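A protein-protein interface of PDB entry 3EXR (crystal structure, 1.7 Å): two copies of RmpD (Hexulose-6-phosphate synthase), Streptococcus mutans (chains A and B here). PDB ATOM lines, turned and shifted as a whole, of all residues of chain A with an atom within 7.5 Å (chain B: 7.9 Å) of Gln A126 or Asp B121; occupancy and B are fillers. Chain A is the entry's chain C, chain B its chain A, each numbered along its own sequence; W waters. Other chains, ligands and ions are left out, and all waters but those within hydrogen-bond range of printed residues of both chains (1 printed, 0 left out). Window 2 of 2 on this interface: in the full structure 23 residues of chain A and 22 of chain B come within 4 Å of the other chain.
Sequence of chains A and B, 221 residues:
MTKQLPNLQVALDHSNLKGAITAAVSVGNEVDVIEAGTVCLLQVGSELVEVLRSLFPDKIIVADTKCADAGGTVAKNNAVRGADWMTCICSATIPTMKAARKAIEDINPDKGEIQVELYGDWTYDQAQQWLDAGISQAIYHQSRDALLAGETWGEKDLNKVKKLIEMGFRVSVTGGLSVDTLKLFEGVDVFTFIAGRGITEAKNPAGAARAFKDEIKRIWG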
ATOM      1  N   CYS A  90      -6.755 -18.751   4.060  1.00  0.00           N
ATOM      2  CA  CYS A  90      -6.917 -18.264   5.431  1.00  0.00           C
ATOM      3  C   CYS A  90      -8.068 -18.924   6.214  1.00  0.00           C
ATOM      4  O   CYS A  90      -8.082 -18.904   7.446  1.00  0.00           O
ATOM      5  CB  CYS A  90      -7.076 -16.738   5.456  1.00  0.00           C
ATOM      6  SG  CYS A  90      -8.397 -16.086   4.407  1.00  0.00           S
ATOM      7  N   SER A  91      -9.028 -19.523   5.516  1.00  0.00           N
ATOM      8  CA  SER A  91     -10.079 -20.253   6.227  1.00  0.00           C
ATOM      9  C   SER A  91      -9.702 -21.677   6.709  1.00  0.00           C
ATOM     10  O   SER A  91     -10.450 -22.303   7.464  1.00  0.00           O
ATOM     11  CB  SER A  91     -11.363 -20.261   5.433  1.00  0.00           C
ATOM     12  OG  SER A  91     -11.137 -20.723   4.162  1.00  0.00           O
ATOM     13  N   ILE A  94      -6.331 -24.024  12.127  1.00  0.00           N
ATOM     14  CA  ILE A  94      -4.987 -24.099  12.687  1.00  0.00           C
ATOM     15  C   ILE A  94      -4.426 -25.526  12.629  1.00  0.00           C
ATOM     16  O   ILE A  94      -3.300 -25.697  12.181  1.00  0.00           O
ATOM     17  CB  ILE A  94      -4.903 -23.457  14.120  1.00  0.00           C
ATOM     18  CG1 ILE A  94      -5.191 -21.949  14.024  1.00  0.00           C
ATOM     19  CG2 ILE A  94      -3.543 -23.746  14.826  1.00  0.00           C
ATOM     20  CD1 ILE A  94      -4.231 -21.137  13.216  1.00  0.00           C
ATOM     21  N   MET A  97      -3.276 -26.076   9.113  1.00  0.00           N
ATOM     22  CA  MET A  97      -2.091 -25.285   8.785  1.00  0.00           C
ATOM     23  C   MET A  97      -0.850 -25.863   9.464  1.00  0.00           C
ATOM     24  O   MET A  97       0.229 -25.969   8.859  1.00  0.00           O
ATOM     25  CB  MET A  97      -2.275 -23.832   9.184  1.00  0.00           C
ATOM     26  CG  MET A  97      -3.305 -23.071   8.378  1.00  0.00           C
ATOM     27  SD  MET A  97      -3.162 -21.330   8.763  1.00  0.00           S
ATOM     28  CE  MET A  97      -4.389 -20.633   7.637  1.00  0.00           C
ATOM     29  N   VAL A 116       0.034 -17.837   4.231  1.00  0.00           N
ATOM     30  CA  VAL A 116      -1.415 -17.738   4.331  1.00  0.00           C
ATOM     31  C   VAL A 116      -1.956 -16.818   3.224  1.00  0.00           C
ATOM     32  O   VAL A 116      -1.631 -15.621   3.156  1.00  0.00           O
ATOM     33  CB  VAL A 116      -1.876 -17.236   5.729  1.00  0.00           C
ATOM     34  CG1 VAL A 116      -3.411 -17.117   5.769  1.00  0.00           C
ATOM     35  CG2 VAL A 116      -1.397 -18.147   6.814  1.00  0.00           C
ATOM     36  N   LEU A 118      -4.690 -14.464   1.810  1.00  0.00           N
ATOM     37  CA  LEU A 118      -5.737 -13.631   2.440  1.00  0.00           C
ATOM     38  C   LEU A 118      -6.900 -13.303   1.501  1.00  0.00           C
ATOM     39  O   LEU A 118      -6.757 -12.539   0.538  1.00  0.00           O
ATOM     40  CB  LEU A 118      -5.151 -12.344   3.028  1.00  0.00           C
ATOM     41  CG  LEU A 118      -4.036 -12.483   4.071  1.00  0.00           C
ATOM     42  CD1 LEU A 118      -3.482 -11.071   4.343  1.00  0.00           C
ATOM     43  CD2 LEU A 118      -4.521 -13.146   5.335  1.00  0.00           C
ATOM     44  N   TYR A 119      -8.059 -13.884   1.803  1.00  0.00           N
ATOM     45  CA  TYR A 119      -9.278 -13.684   1.030  1.00  0.00           C
ATOM     46  C   TYR A 119     -10.427 -13.500   1.997  1.00  0.00           C
ATOM     47  O   TYR A 119     -10.437 -14.082   3.079  1.00  0.00           O
ATOM     48  CB  TYR A 119      -9.585 -14.927   0.161  1.00  0.00           C
ATOM     49  CG  TYR A 119      -8.753 -14.957  -1.101  1.00  0.00           C
ATOM     50  CD1 TYR A 119      -9.256 -14.490  -2.306  1.00  0.00           C
ATOM     51  CD2 TYR A 119      -7.446 -15.440  -1.080  1.00  0.00           C
ATOM     52  CE1 TYR A 119      -8.478 -14.478  -3.465  1.00  0.00           C
ATOM     53  CE2 TYR A 119      -6.661 -15.440  -2.231  1.00  0.00           C
ATOM     54  CZ  TYR A 119      -7.176 -14.946  -3.419  1.00  0.00           C
ATOM     55  OH  TYR A 119      -6.392 -14.970  -4.548  1.00  0.00           O
ATOM     56  N   GLY A 120     -11.391 -12.685   1.594  1.00  0.00           N
ATOM     57  CA  GLY A 120     -12.573 -12.416   2.386  1.00  0.00           C
ATOM     58  C   GLY A 120     -12.293 -11.728   3.716  1.00  0.00           C
ATOM     59  O   GLY A 120     -11.298 -11.001   3.847  1.00  0.00           O
ATOM     60  N   ASP A 121     -13.160 -11.986   4.698  1.00  0.00           N
ATOM     61  CA  ASP A 121     -13.171 -11.278   5.994  1.00  0.00           C
ATOM     62  C   ASP A 121     -12.255 -11.808   7.096  1.00  0.00           C
ATOM     63  O   ASP A 121     -12.729 -12.223   8.171  1.00  0.00           O
ATOM     64  CB  ASP A 121     -14.590 -11.258   6.571  1.00  0.00           C
ATOM     65  CG  ASP A 121     -15.563 -10.501   5.710  1.00  0.00           C
ATOM     66  OD1 ASP A 121     -15.120  -9.656   4.914  1.00  0.00           O
ATOM     67  OD2 ASP A 121     -16.799 -10.718   5.807  1.00  0.00           O
ATOM     68  N   TRP A 122     -10.954 -11.718   6.884  1.00  0.00           N
ATOM     69  CA  TRP A 122      -9.979 -12.160   7.876  1.00  0.00           C
ATOM     70  C   TRP A 122      -9.715 -11.083   8.947  1.00  0.00           C
ATOM     71  O   TRP A 122      -9.904  -9.896   8.692  1.00  0.00           O
ATOM     72  CB  TRP A 122      -8.687 -12.591   7.168  1.00  0.00           C
ATOM     73  CG  TRP A 122      -8.005 -11.480   6.485  1.00  0.00           C
ATOM     74  CD1 TRP A 122      -8.194 -11.058   5.205  1.00  0.00           C
ATOM     75  CD2 TRP A 122      -7.030 -10.605   7.059  1.00  0.00           C
ATOM     76  NE1 TRP A 122      -7.383  -9.970   4.942  1.00  0.00           N
ATOM     77  CE2 TRP A 122      -6.660  -9.673   6.066  1.00  0.00           C
ATOM     78  CE3 TRP A 122      -6.428 -10.528   8.316  1.00  0.00           C
ATOM     79  CZ2 TRP A 122      -5.699  -8.660   6.295  1.00  0.00           C
ATOM     80  CZ3 TRP A 122      -5.479  -9.532   8.547  1.00  0.00           C
ATOM     81  CH2 TRP A 122      -5.124  -8.611   7.534  1.00  0.00           C
ATOM     82  N   THR A 123      -9.269 -11.507  10.129  1.00  0.00           N
ATOM     83  CA  THR A 123      -9.016 -10.601  11.249  1.00  0.00           C
ATOM     84  C   THR A 123      -7.575 -10.672  11.744  1.00  0.00           C
ATOM     85  O   THR A 123      -6.860 -11.642  11.476  1.00  0.00           O
ATOM     86  CB  THR A 123      -9.954 -10.879  12.458  1.00  0.00           C
ATOM     87  OG1 THR A 123      -9.575 -12.096  13.108  1.00  0.00           O
ATOM     88  CG2 THR A 123     -11.415 -11.031  12.042  1.00  0.00           C
ATOM     89  N   TYR A 124      -7.162  -9.653  12.507  1.00  0.00           N
ATOM     90  CA  TYR A 124      -5.827  -9.661  13.108  1.00  0.00           C
ATOM     91  C   TYR A 124      -5.699 -10.699  14.223  1.00  0.00           C
ATOM     92  O   TYR A 124      -4.612 -11.214  14.482  1.00  0.00           O
ATOM     93  CB  TYR A 124      -5.421  -8.256  13.588  1.00  0.00           C
ATOM     94  CG  TYR A 124      -5.294  -7.270  12.448  1.00  0.00           C
ATOM     95  CD1 TYR A 124      -4.277  -7.392  11.502  1.00  0.00           C
ATOM     96  CD2 TYR A 124      -6.203  -6.218  12.297  1.00  0.00           C
ATOM     97  CE1 TYR A 124      -4.163  -6.509  10.454  1.00  0.00           C
ATOM     98  CE2 TYR A 124      -6.093  -5.327  11.247  1.00  0.00           C
ATOM     99  CZ  TYR A 124      -5.068  -5.476  10.322  1.00  0.00           C
ATOM    100  OH  TYR A 124      -4.960  -4.575   9.287  1.00  0.00           O
ATOM    101  N   ASP A 125      -6.814 -11.016  14.873  1.00  0.00           N
ATOM    102  CA  ASP A 125      -6.860 -12.077  15.867  1.00  0.00           C
ATOM    103  C   ASP A 125      -6.540 -13.447  15.262  1.00  0.00           C
ATOM    104  O   ASP A 125      -5.803 -14.220  15.849  1.00  0.00           O
ATOM    105  CB  ASP A 125      -8.233 -12.102  16.540  1.00  0.00           C
ATOM    106  CG  ASP A 125      -8.434 -10.937  17.513  1.00  0.00           C
ATOM    107  OD1 ASP A 125      -7.446 -10.311  17.949  1.00  0.00           O
ATOM    108  OD2 ASP A 125      -9.578 -10.623  17.893  1.00  0.00           O
ATOM    109  N   GLN A 126      -7.116 -13.732  14.095  1.00  0.00           N
ATOM    110  CA  GLN A 126      -6.825 -14.955  13.344  1.00  0.00           C
ATOM    111  C   GLN A 126      -5.356 -14.945  12.958  1.00  0.00           C
ATOM    112  O   GLN A 126      -4.653 -15.934  13.091  1.00  0.00           O
ATOM    113  CB  GLN A 126      -7.699 -15.043  12.082  1.00  0.00           C
ATOM    114  CG  GLN A 126      -9.179 -15.365  12.302  1.00  0.00           C
ATOM    115  CD  GLN A 126     -10.050 -15.110  11.061  1.00  0.00           C
ATOM    116  OE1 GLN A 126      -9.595 -14.540  10.071  1.00  0.00           O
ATOM    117  NE2 GLN A 126     -11.320 -15.521  11.133  1.00  0.00           N
ATOM    118  N   ALA A 127      -4.880 -13.801  12.497  1.00  0.00           N
ATOM    119  CA  ALA A 127      -3.493 -13.700  12.061  1.00  0.00           C
ATOM    120  C   ALA A 127      -2.516 -14.022  13.184  1.00  0.00           C
ATOM    121  O   ALA A 127      -1.477 -14.631  12.958  1.00  0.00           O
ATOM    122  CB  ALA A 127      -3.217 -12.330  11.459  1.00  0.00           C
ATOM    123  N   GLN A 128      -2.854 -13.626  14.409  1.00  0.00           N
ATOM    124  CA  GLN A 128      -1.981 -13.906  15.527  1.00  0.00           C
ATOM    125  C   GLN A 128      -1.946 -15.405  15.796  1.00  0.00           C
ATOM    126  O   GLN A 128      -0.924 -15.947  16.169  1.00  0.00           O
ATOM    127  CB  GLN A 128      -2.433 -13.134  16.777  1.00  0.00           C
ATOM    128  CG  GLN A 128      -1.478 -13.245  17.966  1.00  0.00           C
ATOM    129  CD  GLN A 128      -0.072 -12.784  17.636  1.00  0.00           C
ATOM    130  OE1 GLN A 128       0.135 -11.660  17.136  1.00  0.00           O
ATOM    131  NE2 GLN A 128       0.904 -13.642  17.910  1.00  0.00           N
ATOM    132  N   GLN A 129      -3.062 -16.092  15.573  1.00  0.00           N
ATOM    133  CA  GLN A 129      -3.066 -17.553  15.722  1.00  0.00           C
ATOM    134  C   GLN A 129      -2.154 -18.200  14.671  1.00  0.00           C
ATOM    135  O   GLN A 129      -1.502 -19.194  14.965  1.00  0.00           O
ATOM    136  CB  GLN A 129      -4.466 -18.163  15.620  1.00  0.00           C
ATOM    137  CG  GLN A 129      -5.503 -17.650  16.597  1.00  0.00           C
ATOM    138  CD  GLN A 129      -6.879 -18.146  16.203  1.00  0.00           C
ATOM    139  OE1 GLN A 129      -7.105 -19.352  16.101  1.00  0.00           O
ATOM    140  NE2 GLN A 129      -7.792 -17.224  15.933  1.00  0.00           N
ATOM    141  N   TRP A 130      -2.101 -17.645  13.457  1.00  0.00           N
ATOM    142  CA  TRP A 130      -1.171 -18.176  12.447  1.00  0.00           C
ATOM    143  C   TRP A 130       0.263 -18.067  12.951  1.00  0.00           C
ATOM    144  O   TRP A 130       0.981 -19.059  12.932  1.00  0.00           O
ATOM    145  CB  TRP A 130      -1.326 -17.512  11.070  1.00  0.00           C
ATOM    146  CG  TRP A 130      -2.720 -17.512  10.560  1.00  0.00           C
ATOM    147  CD1 TRP A 130      -3.680 -18.454  10.779  1.00  0.00           C
ATOM    148  CD2 TRP A 130      -3.332 -16.493   9.769  1.00  0.00           C
ATOM    149  NE1 TRP A 130      -4.855 -18.084  10.173  1.00  0.00           N
ATOM    150  CE2 TRP A 130      -4.675 -16.869   9.562  1.00  0.00           C
ATOM    151  CE3 TRP A 130      -2.880 -15.297   9.215  1.00  0.00           C
ATOM    152  CZ2 TRP A 130      -5.555 -16.101   8.827  1.00  0.00           C
ATOM    153  CZ3 TRP A 130      -3.760 -14.515   8.511  1.00  0.00           C
ATOM    154  CH2 TRP A 130      -5.084 -14.914   8.312  1.00  0.00           C
ATOM    155  N   LEU A 131       0.637 -16.899  13.494  1.00  0.00           N
ATOM    156  CA  LEU A 131       1.972 -16.722  14.086  1.00  0.00           C
ATOM    157  C   LEU A 131       2.211 -17.686  15.233  1.00  0.00           C
ATOM    158  O   LEU A 131       3.252 -18.332  15.301  1.00  0.00           O
ATOM    159  CB  LEU A 131       2.172 -15.298  14.567  1.00  0.00           C
ATOM    160  CG  LEU A 131       2.117 -14.170  13.534  1.00  0.00           C
ATOM    161  CD1 LEU A 131       1.919 -12.851  14.274  1.00  0.00           C
ATOM    162  CD2 LEU A 131       3.332 -14.097  12.590  1.00  0.00           C
ATOM    163  N   ASP A 132       1.222 -17.825  16.114  1.00  0.00           N
ATOM    164  CA  ASP A 132       1.377 -18.758  17.236  1.00  0.00           C
ATOM    165  C   ASP A 132       1.582 -20.182  16.737  1.00  0.00           C
ATOM    166  O   ASP A 132       2.255 -20.957  17.385  1.00  0.00           O
ATOM    167  CB  ASP A 132       0.168 -18.687  18.189  1.00  0.00           C
ATOM    168  CG  ASP A 132      -0.005 -17.320  18.808  1.00  0.00           C
ATOM    169  OD1 ASP A 132       0.951 -16.522  18.786  1.00  0.00           O
ATOM    170  OD2 ASP A 132      -1.094 -17.002  19.323  1.00  0.00           O
ATOM    171  N   MET A 167       3.173  -6.923  13.171  1.00  0.00           N
ATOM    172  CA  MET A 167       2.851  -8.143  13.920  1.00  0.00           C
ATOM    173  C   MET A 167       3.914  -9.244  13.841  1.00  0.00           C
ATOM    174  O   MET A 167       3.964 -10.144  14.697  1.00  0.00           O
ATOM    175  CB  MET A 167       1.508  -8.708  13.431  1.00  0.00           C
ATOM    176  CG  MET A 167       0.304  -7.869  13.826  1.00  0.00           C
ATOM    177  SD  MET A 167      -1.236  -8.598  13.267  1.00  0.00           S
ATOM    178  CE  MET A 167      -1.285 -10.030  14.298  1.00  0.00           C
ATOM    179  N   PHE A 169       4.870 -10.585  10.399  1.00  0.00           N
ATOM    180  CA  PHE A 169       4.740 -11.259   9.092  1.00  0.00           C
ATOM    181  C   PHE A 169       5.707 -10.755   8.040  1.00  0.00           C
ATOM    182  O   PHE A 169       5.905  -9.540   7.877  1.00  0.00           O
ATOM    183  CB  PHE A 169       3.305 -11.124   8.519  1.00  0.00           C
ATOM    184  CG  PHE A 169       2.280 -12.025   9.181  1.00  0.00           C
ATOM    185  CD1 PHE A 169       2.131 -13.346   8.772  1.00  0.00           C
ATOM    186  CD2 PHE A 169       1.451 -11.548  10.211  1.00  0.00           C
ATOM    187  CE1 PHE A 169       1.186 -14.166   9.361  1.00  0.00           C
ATOM    188  CE2 PHE A 169       0.490 -12.372  10.824  1.00  0.00           C
ATOM    189  CZ  PHE A 169       0.373 -13.685  10.411  1.00  0.00           C
ATOM    190  N   CYS B  90     -15.505 -20.925   1.065  1.00  0.00           N
ATOM    191  CA  CYS B  90     -16.383 -19.857   1.539  1.00  0.00           C
ATOM    192  C   CYS B  90     -15.677 -18.503   1.627  1.00  0.00           C
ATOM    193  O   CYS B  90     -16.340 -17.470   1.720  1.00  0.00           O
ATOM    194  CB  CYS B  90     -16.997 -20.245   2.888  1.00  0.00           C
ATOM    195  SG  CYS B  90     -15.790 -20.716   4.157  1.00  0.00           S
ATOM    196  N   LEU B 118     -17.693 -25.085   3.484  1.00  0.00           N
ATOM    197  CA  LEU B 118     -17.742 -24.352   4.751  1.00  0.00           C
ATOM    198  C   LEU B 118     -16.567 -24.711   5.634  1.00  0.00           C
ATOM    199  O   LEU B 118     -16.487 -25.841   6.129  1.00  0.00           O
ATOM    200  CB  LEU B 118     -19.074 -24.621   5.457  1.00  0.00           C
ATOM    201  CG  LEU B 118     -20.332 -24.215   4.690  1.00  0.00           C
ATOM    202  CD1 LEU B 118     -21.568 -24.641   5.447  1.00  0.00           C
ATOM    203  CD2 LEU B 118     -20.410 -22.721   4.443  1.00  0.00           C
ATOM    204  N   TYR B 119     -15.635 -23.754   5.761  1.00  0.00           N
ATOM    205  CA  TYR B 119     -14.470 -23.848   6.636  1.00  0.00           C
ATOM    206  C   TYR B 119     -14.310 -22.565   7.433  1.00  0.00           C
ATOM    207  O   TYR B 119     -14.523 -21.467   6.915  1.00  0.00           O
ATOM    208  CB  TYR B 119     -13.191 -24.082   5.824  1.00  0.00           C
ATOM    209  CG  TYR B 119     -13.068 -25.510   5.314  1.00  0.00           C
ATOM    210  CD1 TYR B 119     -12.346 -26.461   6.019  1.00  0.00           C
ATOM    211  CD2 TYR B 119     -13.746 -25.932   4.167  1.00  0.00           C
ATOM    212  CE1 TYR B 119     -12.241 -27.756   5.572  1.00  0.00           C
ATOM    213  CE2 TYR B 119     -13.668 -27.242   3.722  1.00  0.00           C
ATOM    214  CZ  TYR B 119     -12.907 -28.151   4.428  1.00  0.00           C
ATOM    215  OH  TYR B 119     -12.791 -29.454   3.992  1.00  0.00           O
ATOM    216  N   GLY B 120     -13.869 -22.718   8.678  1.00  0.00           N
ATOM    217  CA  GLY B 120     -13.551 -21.582   9.537  1.00  0.00           C
ATOM    218  C   GLY B 120     -14.779 -20.810   9.976  1.00  0.00           C
ATOM    219  O   GLY B 120     -15.882 -21.382  10.028  1.00  0.00           O
ATOM    220  N   ASP B 121     -14.592 -19.524  10.253  1.00  0.00           N
ATOM    221  CA  ASP B 121     -15.614 -18.674  10.882  1.00  0.00           C
ATOM    222  C   ASP B 121     -16.576 -17.977   9.923  1.00  0.00           C
ATOM    223  O   ASP B 121     -16.718 -16.732   9.927  1.00  0.00           O
ATOM    224  CB  ASP B 121     -14.915 -17.598  11.724  1.00  0.00           C
ATOM    225  CG  ASP B 121     -14.107 -18.178  12.839  1.00  0.00           C
ATOM    226  OD1 ASP B 121     -14.587 -19.142  13.486  1.00  0.00           O
ATOM    227  OD2 ASP B 121     -12.983 -17.701  13.104  1.00  0.00           O
ATOM    228  N   TRP B 122     -17.266 -18.755   9.114  1.00  0.00           N
ATOM    229  CA  TRP B 122     -18.272 -18.192   8.224  1.00  0.00           C
ATOM    230  C   TRP B 122     -19.516 -17.820   9.017  1.00  0.00           C
ATOM    231  O   TRP B 122     -19.761 -18.388  10.086  1.00  0.00           O
ATOM    232  CB  TRP B 122     -18.620 -19.173   7.096  1.00  0.00           C
ATOM    233  CG  TRP B 122     -19.196 -20.420   7.604  1.00  0.00           C
ATOM    234  CD1 TRP B 122     -18.516 -21.521   7.997  1.00  0.00           C
ATOM    235  CD2 TRP B 122     -20.588 -20.694   7.841  1.00  0.00           C
ATOM    236  NE1 TRP B 122     -19.399 -22.478   8.451  1.00  0.00           N
ATOM    237  CE2 TRP B 122     -20.675 -21.996   8.359  1.00  0.00           C
ATOM    238  CE3 TRP B 122     -21.769 -19.978   7.630  1.00  0.00           C
ATOM    239  CZ2 TRP B 122     -21.884 -22.587   8.688  1.00  0.00           C
ATOM    240  CZ3 TRP B 122     -22.965 -20.549   7.976  1.00  0.00           C
ATOM    241  CH2 TRP B 122     -23.019 -21.855   8.490  1.00  0.00           C
ATOM    242  N   THR B 123     -20.281 -16.868   8.500  1.00  0.00           N
ATOM    243  CA  THR B 123     -21.483 -16.370   9.166  1.00  0.00           C
ATOM    244  C   THR B 123     -22.758 -16.592   8.328  1.00  0.00           C
ATOM    245  O   THR B 123     -22.700 -16.819   7.112  1.00  0.00           O
ATOM    246  CB  THR B 123     -21.366 -14.849   9.434  1.00  0.00           C
ATOM    247  OG1 THR B 123     -21.370 -14.150   8.186  1.00  0.00           O
ATOM    248  CG2 THR B 123     -20.081 -14.491  10.168  1.00  0.00           C
ATOM    249  N   TYR B 124     -23.917 -16.498   8.980  1.00  0.00           N
ATOM    250  CA  TYR B 124     -25.190 -16.549   8.274  1.00  0.00           C
ATOM    251  C   TYR B 124     -25.434 -15.298   7.386  1.00  0.00           C
ATOM    252  O   TYR B 124     -26.161 -15.368   6.394  1.00  0.00           O
ATOM    253  CB  TYR B 124     -26.328 -16.743   9.261  1.00  0.00           C
ATOM    254  CG  TYR B 124     -26.274 -18.086   9.973  1.00  0.00           C
ATOM    255  CD1 TYR B 124     -26.478 -19.265   9.260  1.00  0.00           C
ATOM    256  CD2 TYR B 124     -26.032 -18.177  11.349  1.00  0.00           C
ATOM    257  CE1 TYR B 124     -26.444 -20.513   9.896  1.00  0.00           C
ATOM    258  CE2 TYR B 124     -26.001 -19.432  12.000  1.00  0.00           C
ATOM    259  CZ  TYR B 124     -26.193 -20.588  11.257  1.00  0.00           C
ATOM    260  OH  TYR B 124     -26.186 -21.837  11.864  1.00  0.00           O
ATOM    261  N   GLN B 126     -23.016 -13.904   5.635  1.00  0.00           N
ATOM    262  CA  GLN B 126     -22.311 -14.342   4.424  1.00  0.00           C
ATOM    263  C   GLN B 126     -23.164 -15.346   3.650  1.00  0.00           C
ATOM    264  O   GLN B 126     -23.316 -15.235   2.427  1.00  0.00           O
ATOM    265  CB  GLN B 126     -20.952 -14.952   4.783  1.00  0.00           C
ATOM    266  CG  GLN B 126     -19.935 -13.978   5.369  1.00  0.00           C
ATOM    267  CD  GLN B 126     -18.661 -14.673   5.863  1.00  0.00           C
ATOM    268  OE1 GLN B 126     -18.687 -15.838   6.242  1.00  0.00           O
ATOM    269  NE2 GLN B 126     -17.548 -13.949   5.857  1.00  0.00           N
ATOM    270  N   TRP B 130     -24.431 -15.498  -0.387  1.00  0.00           N
ATOM    271  CA  TRP B 130     -24.282 -16.551  -1.378  1.00  0.00           C
ATOM    272  C   TRP B 130     -25.626 -16.804  -2.065  1.00  0.00           C
ATOM    273  O   TRP B 130     -25.699 -16.847  -3.286  1.00  0.00           O
ATOM    274  CB  TRP B 130     -23.717 -17.874  -0.776  1.00  0.00           C
ATOM    275  CG  TRP B 130     -22.471 -17.686   0.055  1.00  0.00           C
ATOM    276  CD1 TRP B 130     -21.483 -16.772  -0.142  1.00  0.00           C
ATOM    277  CD2 TRP B 130     -22.104 -18.427   1.219  1.00  0.00           C
ATOM    278  NE1 TRP B 130     -20.527 -16.885   0.837  1.00  0.00           N
ATOM    279  CE2 TRP B 130     -20.895 -17.884   1.699  1.00  0.00           C
ATOM    280  CE3 TRP B 130     -22.705 -19.479   1.937  1.00  0.00           C
ATOM    281  CZ2 TRP B 130     -20.246 -18.380   2.833  1.00  0.00           C
ATOM    282  CZ3 TRP B 130     -22.071 -19.948   3.077  1.00  0.00           C
ATOM    283  CH2 TRP B 130     -20.857 -19.403   3.512  1.00  0.00           C
ATOM    284  N   LYS B 160     -26.805 -26.090  13.007  1.00  0.00           N
ATOM    285  CA  LYS B 160     -26.305 -25.277  11.899  1.00  0.00           C
ATOM    286  C   LYS B 160     -26.771 -25.831  10.551  1.00  0.00           C
ATOM    287  O   LYS B 160     -27.190 -25.094   9.665  1.00  0.00           O
ATOM    288  CB  LYS B 160     -24.781 -25.130  11.972  1.00  0.00           C
ATOM    289  CG  LYS B 160     -24.306 -24.474  13.284  1.00  0.00           C
ATOM    290  CD  LYS B 160     -22.881 -23.964  13.203  1.00  0.00           C
ATOM    291  CE  LYS B 160     -22.788 -22.720  12.355  1.00  0.00           C
ATOM    292  NZ  LYS B 160     -21.401 -22.139  12.442  1.00  0.00           N
HETATM  293  O   HOH W   1     -14.896 -14.403   4.197  1.00  0.00           O
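O of Tyr B119 is in hydrogen-bond range of SG of Cys B90, 3.1 Å away.
N of Thr B123 sits at hydrogen-bond distance from OE1 of Gln B126, 2.9 Å away.
The backbone NH of Thr A123 lies within hydrogen-bond range of the side-chain amide oxygen of Gln A126 (3.1 Å).
OD2 of Asp B121 sits at hydrogen-bond distance from NE2 of Gln A126, at 3.4 Å.
The side-chain carboxylate (OD2) of Asp A121 lies within hydrogen-bond range of the side-chain amide nitrogen (NE2) of Gln B126.
Of the 22 printed residues of chain A, 3 touch a printed residue of chain B.
Of the 11 printed residues of chain B, 4 touch a printed residue of chain A.
Among the printed residues, 4 pairs touch across the chains.
Among the printed residues, no Asp or Glu carboxylate lies within 4 Å of a Lys or Arg side-chain nitrogen of the other chain.
Water W1 bridges N of Asp A121 and NE2 of Gln B126.
Among the printed residues, merely in contact across the chains: Ser A91 with Gly B120 and Ser A91 with Tyr B119.
Gln A126 touches just one residue of chain B: Asp B121 (3.4 Å).
Asp B121 touches one residue of chain A.
Of the printed residues of chain A, Gly B120 touches Ser A91.
Of the printed residues of chain A, Gln B126 touches Asp A121 (3.3 Å).
Leu A118 touches none of the printed residues of chain B.
Thr A123 touches none of the printed residues of chain B.
The nearest residue of chain B that does not touch Gln A126 is Gly B120 (6.4 Å).
The nearest residue of chain A that does not touch Asp B121 is Ser A91 (5.7 Å).
The nearest printed residue of chain A that does not touch Gln B126 is Gly A120 (6.1 Å).
Asp A121 touches Gln B126, and with the chains exchanged Gln A126 touches Asp B121.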
